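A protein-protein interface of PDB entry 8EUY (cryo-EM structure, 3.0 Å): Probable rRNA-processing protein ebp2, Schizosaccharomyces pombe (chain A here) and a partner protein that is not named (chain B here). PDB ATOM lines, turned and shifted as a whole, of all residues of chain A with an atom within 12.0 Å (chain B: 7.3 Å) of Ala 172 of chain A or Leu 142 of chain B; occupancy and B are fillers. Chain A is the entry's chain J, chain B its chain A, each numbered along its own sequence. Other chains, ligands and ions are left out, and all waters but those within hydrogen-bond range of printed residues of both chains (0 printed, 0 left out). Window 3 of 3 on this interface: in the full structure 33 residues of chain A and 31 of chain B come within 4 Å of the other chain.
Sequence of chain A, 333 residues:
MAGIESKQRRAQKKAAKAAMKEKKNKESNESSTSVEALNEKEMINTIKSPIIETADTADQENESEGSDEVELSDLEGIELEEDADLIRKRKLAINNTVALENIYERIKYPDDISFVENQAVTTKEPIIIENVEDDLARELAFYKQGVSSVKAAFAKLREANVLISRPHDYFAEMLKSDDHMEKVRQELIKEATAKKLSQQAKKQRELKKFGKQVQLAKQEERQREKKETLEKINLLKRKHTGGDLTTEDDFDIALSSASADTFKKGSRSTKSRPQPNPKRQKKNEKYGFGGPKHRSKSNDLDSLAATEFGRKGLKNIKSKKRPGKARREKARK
The backbone NH (N) of Lys 176 of chain A sits at hydrogen-bond distance from the backbone carbonyl oxygen (O) of Ala 141 of chain B, 3.4 Å away. The backbone NH (N) of Lys 143 of chain B sits close to the backbone NH (N) of Leu 175 of chain A. The backbone carbonyl oxygen (O) of Glu 173 of chain A lies within hydrogen-bond range of the backbone NH (N) of Lys 143 of chain B, 2.4 Å away. The backbone NH of Leu 175 of chain A sits at hydrogen-bond distance from the backbone carbonyl oxygen of Ala 141 of chain B, 2.6 Å away.
O of Leu 142 of chain B sits at hydrogen-bond distance from OG of Ser 145 of chain B (2.5 Å). SD of Met 67 of chain B sits at hydrogen-bond distance from OG of Ser 66 of chain B (2.8 Å). The backbone carbonyl oxygen of Phe 184 of chain B sits at hydrogen-bond distance from the backbone NH of Arg 146 of chain B (3.4 Å). NH2 of Arg 187 of chain B sits at hydrogen-bond distance from O of Met 67 of chain B, 3.1 Å away.
Among the printed residues, pairs that only touch across the chains: Glu 173 of chain A with Leu 142 of chain B (3.2 Å), Ser 165 of chain A with Phe 184 of chain B (3.4 Å), Met 174 of chain A with Ala 141 of chain B (3.4 Å), Met 174 of chain A with Lys 143 of chain B (3.4 Å), Ala 172 of chain A with Leu 142 of chain B (3.5 Å), Ile 164 of chain A with Ile 185 of chain B (3.5 Å), Leu 175 of chain A with Met 67 of chain B (3.6 Å), Leu 175 of chain A with Leu 142 of chain B (3.6 Å), Arg 166 of chain A with Phe 184 of chain B (3.6 Å), Lys 176 of chain A with Asn 140 of chain B (3.7 Å), Met 174 of chain A with Leu 142 of chain B (3.8 Å) and Met 174 of chain A with Asn 140 of chain B (3.8 Å).
Of the printed residues of chain B, Ile 164 of chain A touches Ile 185. Printed residues of chain B within 4 Å of Ser 165 of chain A: Phe 184. Printed residues of chain B within 4 Å of Ala 172 of chain A: Leu 142 (3.5 Å). Asn 140 of chain B touches just these residues of chain A: Met 174 and Lys 176. Ala 141 of chain B touches just these residues of chain A: Met 174, Leu 175 and Lys 176. Leu 142 of chain B touches just these residues of chain A: Ala 172 (3.5 Å), Glu 173 (3.2 Å), Met 174 (3.8 Å) and Leu 175 (3.6 Å). Printed residues of chain A within 4 Å of Lys 143 of chain B: Glu 173, Met 174 and Leu 175. No residue of chain A comes within 4 Å of Gly 144 of chain B. No residue of chain A comes within 4 Å of Ser 145 of chain B. Asp 186 of chain B touches none of the printed residues of chain A. The nearest printed residue of chain A that does not touch Phe 184 of chain B is Pro 167 of chain A (4.02 Å).
Hydrophobic or aromatic side chains of chain A within 4 Å of the printed part of chain B: Ala 172, Met 174 and Leu 175. Of the 16 printed residues of chain B, 7 touch a printed residue of chain A. Printed residues of chain B that touch a printed residue of chain A: Met 67, Asn 140, Ala 141, Leu 142, Lys 143, Phe 184 and Ile 185. Among the printed residues, no Asp or Glu carboxylate lies within 4 Å of a Lys or Arg side-chain nitrogen of the other chain.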
ATOM      1  N   LEU A 163      13.615  12.539  -5.051  1.00  0.00           N
ATOM      2  CA  LEU A 163      12.612  13.597  -5.044  1.00  0.00           C
ATOM      3  C   LEU A 163      11.243  13.013  -4.713  1.00  0.00           C
ATOM      4  O   LEU A 163      10.734  12.152  -5.439  1.00  0.00           O
ATOM      5  CB  LEU A 163      12.581  14.306  -6.396  1.00  0.00           C
ATOM      6  N   ILE A 164      10.651  13.480  -3.619  1.00  0.00           N
ATOM      7  CA  ILE A 164       9.348  13.003  -3.167  1.00  0.00           C
ATOM      8  C   ILE A 164       8.225  13.907  -3.651  1.00  0.00           C
ATOM      9  O   ILE A 164       7.264  13.442  -4.264  1.00  0.00           O
ATOM     10  CB  ILE A 164       9.335  12.866  -1.628  1.00  0.00           C
ATOM     11  N   SER A 165       8.326  15.205  -3.377  1.00  0.00           N
ATOM     12  CA  SER A 165       7.304  16.144  -3.817  1.00  0.00           C
ATOM     13  C   SER A 165       7.319  16.281  -5.334  1.00  0.00           C
ATOM     14  O   SER A 165       8.381  16.364  -5.958  1.00  0.00           O
ATOM     15  CB  SER A 165       7.520  17.508  -3.163  1.00  0.00           C
ATOM     16  N   ARG A 166       6.131  16.302  -5.927  1.00  0.00           N
ATOM     17  CA  ARG A 166       6.012  16.457  -7.371  1.00  0.00           C
ATOM     18  C   ARG A 166       6.233  17.915  -7.751  1.00  0.00           C
ATOM     19  O   ARG A 166       5.522  18.791  -7.244  1.00  0.00           O
ATOM     20  CB  ARG A 166       4.643  15.991  -7.848  1.00  0.00           C
ATOM     21  N   PRO A 167       7.198  18.222  -8.616  1.00  0.00           N
ATOM     22  CA  PRO A 167       7.408  19.618  -9.015  1.00  0.00           C
ATOM     23  C   PRO A 167       6.197  20.176  -9.749  1.00  0.00           C
ATOM     24  O   PRO A 167       5.534  19.476 -10.517  1.00  0.00           O
ATOM     25  CB  PRO A 167       8.636  19.546  -9.927  1.00  0.00           C
ATOM     26  N   HIS A 168       5.910  21.456  -9.499  1.00  0.00           N
ATOM     27  CA  HIS A 168       4.797  22.109 -10.177  1.00  0.00           C
ATOM     28  C   HIS A 168       5.097  22.346 -11.652  1.00  0.00           C
ATOM     29  O   HIS A 168       4.188  22.279 -12.487  1.00  0.00           O
ATOM     30  CB  HIS A 168       4.459  23.430  -9.485  1.00  0.00           C
ATOM     31  N   ASP A 169       6.358  22.631 -11.988  1.00  0.00           N
ATOM     32  CA  ASP A 169       6.722  22.863 -13.381  1.00  0.00           C
ATOM     33  C   ASP A 169       6.530  21.607 -14.221  1.00  0.00           C
ATOM     34  O   ASP A 169       6.071  21.683 -15.368  1.00  0.00           O
ATOM     35  CB  ASP A 169       8.168  23.352 -13.471  1.00  0.00           C
ATOM     36  N   TYR A 170       6.882  20.446 -13.674  1.00  0.00           N
ATOM     37  CA  TYR A 170       6.726  19.196 -14.404  1.00  0.00           C
ATOM     38  C   TYR A 170       5.254  18.923 -14.690  1.00  0.00           C
ATOM     39  O   TYR A 170       4.393  19.082 -13.821  1.00  0.00           O
ATOM     40  CB  TYR A 170       7.331  18.038 -13.608  1.00  0.00           C
ATOM     41  N   PHE A 171       4.970  18.508 -15.922  1.00  0.00           N
ATOM     42  CA  PHE A 171       3.608  18.231 -16.375  1.00  0.00           C
ATOM     43  C   PHE A 171       3.553  16.787 -16.863  1.00  0.00           C
ATOM     44  O   PHE A 171       3.989  16.484 -17.978  1.00  0.00           O
ATOM     45  CB  PHE A 171       3.186  19.207 -17.470  1.00  0.00           C
ATOM     46  N   ALA A 172       3.019  15.901 -16.030  1.00  0.00           N
ATOM     47  CA  ALA A 172       2.860  14.493 -16.358  1.00  0.00           C
ATOM     48  C   ALA A 172       1.379  14.139 -16.398  1.00  0.00           C
ATOM     49  O   ALA A 172       0.519  14.901 -15.948  1.00  0.00           O
ATOM     50  CB  ALA A 172       3.598  13.602 -15.350  1.00  0.00           C
ATOM     51  N   GLU A 173       1.087  12.965 -16.952  1.00  0.00           N
ATOM     52  CA  GLU A 173      -0.290  12.499 -17.036  1.00  0.00           C
ATOM     53  C   GLU A 173      -0.854  12.248 -15.644  1.00  0.00           C
ATOM     54  O   GLU A 173      -0.175  11.709 -14.767  1.00  0.00           O
ATOM     55  CB  GLU A 173      -0.369  11.224 -17.875  1.00  0.00           C
ATOM     56  N   MET A 174      -2.109  12.645 -15.445  1.00  0.00           N
ATOM     57  CA  MET A 174      -2.792  12.496 -14.168  1.00  0.00           C
ATOM     58  C   MET A 174      -3.796  11.355 -14.259  1.00  0.00           C
ATOM     59  O   MET A 174      -4.633  11.331 -15.167  1.00  0.00           O
ATOM     60  CB  MET A 174      -3.498  13.793 -13.769  1.00  0.00           C
ATOM     61  N   LEU A 175      -3.701  10.411 -13.320  1.00  0.00           N
ATOM     62  CA  LEU A 175      -4.629   9.286 -13.305  1.00  0.00           C
ATOM     63  C   LEU A 175      -6.056   9.746 -13.029  1.00  0.00           C
ATOM     64  O   LEU A 175      -7.003   9.265 -13.664  1.00  0.00           O
ATOM     65  CB  LEU A 175      -4.186   8.258 -12.264  1.00  0.00           C
ATOM     66  N   LYS A 176      -6.228  10.670 -12.088  1.00  0.00           N
ATOM     67  CA  LYS A 176      -7.556  11.169 -11.760  1.00  0.00           C
ATOM     68  C   LYS A 176      -8.132  11.971 -12.921  1.00  0.00           C
ATOM     69  O   LYS A 176      -7.425  12.738 -13.580  1.00  0.00           O
ATOM     70  CB  LYS A 176      -7.502  12.034 -10.500  1.00  0.00           C
ATOM     71  N   SER A 177      -9.427  11.788 -13.166  1.00  0.00           N
ATOM     72  CA  SER A 177     -10.105  12.483 -14.253  1.00  0.00           C
ATOM     73  C   SER A 177     -10.431  13.908 -13.825  1.00  0.00           C
ATOM     74  O   SER A 177     -11.192  14.119 -12.874  1.00  0.00           O
ATOM     75  CB  SER A 177     -11.374  11.736 -14.655  1.00  0.00           C
ATOM     76  N   ASP A 178      -9.850  14.886 -14.525  1.00  0.00           N
ATOM     77  CA  ASP A 178     -10.141  16.284 -14.224  1.00  0.00           C
ATOM     78  C   ASP A 178     -11.587  16.629 -14.558  1.00  0.00           C
ATOM     79  O   ASP A 178     -12.224  17.413 -13.845  1.00  0.00           O
ATOM     80  CB  ASP A 178      -9.181  17.196 -14.987  1.00  0.00           C
ATOM     81  N   SER B  66      -5.708   1.921 -15.528  1.00  0.00           N
ATOM     82  CA  SER B  66      -5.201   3.287 -15.622  1.00  0.00           C
ATOM     83  C   SER B  66      -4.219   3.597 -14.499  1.00  0.00           C
ATOM     84  O   SER B  66      -3.187   4.237 -14.729  1.00  0.00           O
ATOM     85  CB  SER B  66      -6.364   4.279 -15.608  1.00  0.00           C
ATOM     86  OG  SER B  66      -6.914   4.402 -14.308  1.00  0.00           O
ATOM     87  N   MET B  67      -4.516   3.151 -13.279  1.00  0.00           N
ATOM     88  CA  MET B  67      -3.606   3.357 -12.160  1.00  0.00           C
ATOM     89  C   MET B  67      -2.471   2.344 -12.127  1.00  0.00           C
ATOM     90  O   MET B  67      -1.654   2.384 -11.200  1.00  0.00           O
ATOM     91  CB  MET B  67      -4.367   3.310 -10.831  1.00  0.00           C
ATOM     92  CG  MET B  67      -5.826   3.723 -10.914  1.00  0.00           C
ATOM     93  SD  MET B  67      -6.085   5.256 -11.824  1.00  0.00           S
ATOM     94  CE  MET B  67      -7.776   5.639 -11.370  1.00  0.00           C
ATOM     95  N   ASN B 140      -6.419  13.862  -6.929  1.00  0.00           N
ATOM     96  CA  ASN B 140      -5.641  14.210  -8.118  1.00  0.00           C
ATOM     97  C   ASN B 140      -4.267  13.561  -7.977  1.00  0.00           C
ATOM     98  O   ASN B 140      -3.396  14.089  -7.280  1.00  0.00           O
ATOM     99  CB  ASN B 140      -5.532  15.719  -8.283  1.00  0.00           C
ATOM    100  CG  ASN B 140      -4.629  16.116  -9.435  1.00  0.00           C
ATOM    101  OD1 ASN B 140      -4.515  15.395 -10.426  1.00  0.00           O
ATOM    102  ND2 ASN B 140      -3.982  17.270  -9.309  1.00  0.00           N
ATOM    103  N   ALA B 141      -4.079  12.428  -8.647  1.00  0.00           N
ATOM    104  CA  ALA B 141      -2.823  11.691  -8.620  1.00  0.00           C
ATOM    105  C   ALA B 141      -2.282  11.544 -10.034  1.00  0.00           C
ATOM    106  O   ALA B 141      -3.040  11.295 -10.977  1.00  0.00           O
ATOM    107  CB  ALA B 141      -3.002  10.311  -7.982  1.00  0.00           C
ATOM    108  N   LEU B 142      -0.969  11.703 -10.176  1.00  0.00           N
ATOM    109  CA  LEU B 142      -0.336  11.566 -11.480  1.00  0.00           C
ATOM    110  C   LEU B 142      -0.390  10.119 -11.951  1.00  0.00           C
ATOM    111  O   LEU B 142      -0.161   9.186 -11.176  1.00  0.00           O
ATOM    112  CB  LEU B 142       1.114  12.045 -11.419  1.00  0.00           C
ATOM    113  CG  LEU B 142       1.321  13.550 -11.238  1.00  0.00           C
ATOM    114  CD1 LEU B 142       2.716  13.841 -10.707  1.00  0.00           C
ATOM    115  CD2 LEU B 142       1.078  14.285 -12.548  1.00  0.00           C
ATOM    116  N   LYS B 143      -0.698   9.935 -13.233  1.00  0.00           N
ATOM    117  CA  LYS B 143      -0.772   8.596 -13.800  1.00  0.00           C
ATOM    118  C   LYS B 143       0.623   7.990 -13.893  1.00  0.00           C
ATOM    119  O   LYS B 143       1.549   8.613 -14.420  1.00  0.00           O
ATOM    120  CB  LYS B 143      -1.426   8.637 -15.179  1.00  0.00           C
ATOM    121  CG  LYS B 143      -1.779   7.268 -15.738  1.00  0.00           C
ATOM    122  CD  LYS B 143      -2.696   7.386 -16.944  1.00  0.00           C
ATOM    123  CE  LYS B 143      -3.134   6.018 -17.444  1.00  0.00           C
ATOM    124  NZ  LYS B 143      -4.313   6.107 -18.348  1.00  0.00           N
ATOM    125  N   GLY B 144       0.769   6.770 -13.383  1.00  0.00           N
ATOM    126  CA  GLY B 144       2.054   6.109 -13.342  1.00  0.00           C
ATOM    127  C   GLY B 144       2.929   6.485 -12.168  1.00  0.00           C
ATOM    128  O   GLY B 144       4.024   5.926 -12.032  1.00  0.00           O
ATOM    129  N   SER B 145       2.489   7.410 -11.320  1.00  0.00           N
ATOM    130  CA  SER B 145       3.273   7.795 -10.156  1.00  0.00           C
ATOM    131  C   SER B 145       3.328   6.655  -9.148  1.00  0.00           C
ATOM    132  O   SER B 145       2.323   5.991  -8.882  1.00  0.00           O
ATOM    133  CB  SER B 145       2.679   9.044  -9.508  1.00  0.00           C
ATOM    134  OG  SER B 145       1.326   8.834  -9.147  1.00  0.00           O
ATOM    135  N   ARG B 146       4.507   6.431  -8.588  1.00  0.00           N
ATOM    136  CA  ARG B 146       4.684   5.357  -7.618  1.00  0.00           C
ATOM    137  C   ARG B 146       3.986   5.717  -6.314  1.00  0.00           C
ATOM    138  O   ARG B 146       4.313   6.748  -5.712  1.00  0.00           O
ATOM    139  CB  ARG B 146       6.167   5.099  -7.375  1.00  0.00           C
ATOM    140  CG  ARG B 146       6.941   4.700  -8.619  1.00  0.00           C
ATOM    141  CD  ARG B 146       8.372   4.324  -8.275  1.00  0.00           C
ATOM    142  NE  ARG B 146       8.437   3.113  -7.465  1.00  0.00           N
ATOM    143  CZ  ARG B 146       9.126   3.002  -6.337  1.00  0.00           C
ATOM    144  NH1 ARG B 146       9.822   4.016  -5.849  1.00  0.00           N
ATOM    145  NH2 ARG B 146       9.116   1.844  -5.683  1.00  0.00           N
ATOM    146  N   LYS B 182       6.305   7.087 -12.990  1.00  0.00           N
ATOM    147  CA  LYS B 182       6.773   8.400 -12.580  1.00  0.00           C
ATOM    148  C   LYS B 182       7.453   8.310 -11.225  1.00  0.00           C
ATOM    149  O   LYS B 182       6.860   7.776 -10.277  1.00  0.00           O
ATOM    150  CB  LYS B 182       5.610   9.395 -12.512  1.00  0.00           C
ATOM    151  CG  LYS B 182       4.611   9.270 -13.651  1.00  0.00           C
ATOM    152  CD  LYS B 182       5.238   9.633 -14.986  1.00  0.00           C
ATOM    153  CE  LYS B 182       4.187   9.709 -16.082  1.00  0.00           C
ATOM    154  NZ  LYS B 182       4.756  10.183 -17.372  1.00  0.00           N
ATOM    155  N   PHE B 184       7.867  10.565  -9.078  1.00  0.00           N
ATOM    156  CA  PHE B 184       7.160  11.365  -8.092  1.00  0.00           C
ATOM    157  C   PHE B 184       6.040  10.554  -7.445  1.00  0.00           C
ATOM    158  O   PHE B 184       5.532   9.581  -8.008  1.00  0.00           O
ATOM    159  CB  PHE B 184       6.589  12.628  -8.736  1.00  0.00           C
ATOM    160  CG  PHE B 184       7.637  13.553  -9.284  1.00  0.00           C
ATOM    161  CD1 PHE B 184       8.580  14.127  -8.447  1.00  0.00           C
ATOM    162  CD2 PHE B 184       7.677  13.852 -10.635  1.00  0.00           C
ATOM    163  CE1 PHE B 184       9.545  14.980  -8.948  1.00  0.00           C
ATOM    164  CE2 PHE B 184       8.640  14.705 -11.143  1.00  0.00           C
ATOM    165  CZ  PHE B 184       9.575  15.269 -10.298  1.00  0.00           C
ATOM    166  N   ILE B 185       5.656  10.973  -6.241  1.00  0.00           N
ATOM    167  CA  ILE B 185       4.614  10.311  -5.466  1.00  0.00           C
ATOM    168  C   ILE B 185       3.460  11.286  -5.286  1.00  0.00           C
ATOM    169  O   ILE B 185       3.658  12.414  -4.820  1.00  0.00           O
ATOM    170  CB  ILE B 185       5.138   9.828  -4.102  1.00  0.00           C
ATOM    171  CG1 ILE B 185       6.369   8.937  -4.288  1.00  0.00           C
ATOM    172  CG2 ILE B 185       4.047   9.085  -3.344  1.00  0.00           C
ATOM    173  CD1 ILE B 185       7.076   8.596  -2.996  1.00  0.00           C
ATOM    174  N   ASP B 186       2.254  10.848  -5.657  1.00  0.00           N
ATOM    175  CA  ASP B 186       1.070  11.685  -5.515  1.00  0.00           C
ATOM    176  C   ASP B 186      -0.136  10.914  -4.991  1.00  0.00           C
ATOM    177  O   ASP B 186      -1.239  11.474  -4.954  1.00  0.00           O
ATOM    178  CB  ASP B 186       0.715  12.348  -6.852  1.00  0.00           C
ATOM    179  CG  ASP B 186       0.094  13.719  -6.675  1.00  0.00           C
ATOM    180  OD1 ASP B 186       0.143  14.253  -5.547  1.00  0.00           O
ATOM    181  OD2 ASP B 186      -0.444  14.261  -7.663  1.00  0.00           O
ATOM    182  N   ARG B 187       0.032   9.656  -4.588  1.00  0.00           N
ATOM    183  CA  ARG B 187      -1.085   8.870  -4.087  1.00  0.00           C
ATOM    184  C   ARG B 187      -0.574   7.860  -3.070  1.00  0.00           C
ATOM    185  O   ARG B 187       0.604   7.494  -3.062  1.00  0.00           O
ATOM    186  CB  ARG B 187      -1.828   8.158  -5.223  1.00  0.00           C
ATOM    187  CG  ARG B 187      -0.926   7.367  -6.152  1.00  0.00           C
ATOM    188  CD  ARG B 187      -1.731   6.680  -7.241  1.00  0.00           C
ATOM    189  NE  ARG B 187      -0.889   5.869  -8.112  1.00  0.00           N
ATOM    190  CZ  ARG B 187      -0.882   4.543  -8.122  1.00  0.00           C
ATOM    191  NH1 ARG B 187      -1.665   3.843  -7.319  1.00  0.00           N
ATOM    192  NH2 ARG B 187      -0.068   3.905  -8.958  1.00  0.00           N
ATOM    193  N   GLU B 204      -4.753  11.051  -1.609  1.00  0.00           N
ATOM    194  CA  GLU B 204      -3.896  12.036  -2.256  1.00  0.00           C
ATOM    195  C   GLU B 204      -3.119  12.803  -1.198  1.00  0.00           C
ATOM    196  O   GLU B 204      -3.690  13.222  -0.184  1.00  0.00           O
ATOM    197  CB  GLU B 204      -4.719  13.004  -3.113  1.00  0.00           C
ATOM    198  CG  GLU B 204      -3.907  13.783  -4.130  1.00  0.00           C
ATOM    199  CD  GLU B 204      -3.498  15.152  -3.624  1.00  0.00           C
ATOM    200  OE1 GLU B 204      -4.102  15.628  -2.640  1.00  0.00           O
ATOM    201  OE2 GLU B 204      -2.576  15.754  -4.213  1.00  0.00           O
ATOM    202  N   ILE B 221      -8.649   9.349  -3.691  1.00  0.00           N
ATOM    203  CA  ILE B 221      -8.475   9.336  -5.139  1.00  0.00           C
ATOM    204  C   ILE B 221      -9.767   8.918  -5.831  1.00  0.00           C
ATOM    205  O   ILE B 221     -10.144   9.483  -6.865  1.00  0.00           O
ATOM    206  CB  ILE B 221      -7.299   8.422  -5.528  1.00  0.00           C
ATOM    207  CG1 ILE B 221      -5.996   8.950  -4.924  1.00  0.00           C
ATOM    208  CG2 ILE B 221      -7.178   8.315  -7.040  1.00  0.00           C
ATOM    209  CD1 ILE B 221      -5.633  10.341  -5.387  1.00  0.00           C
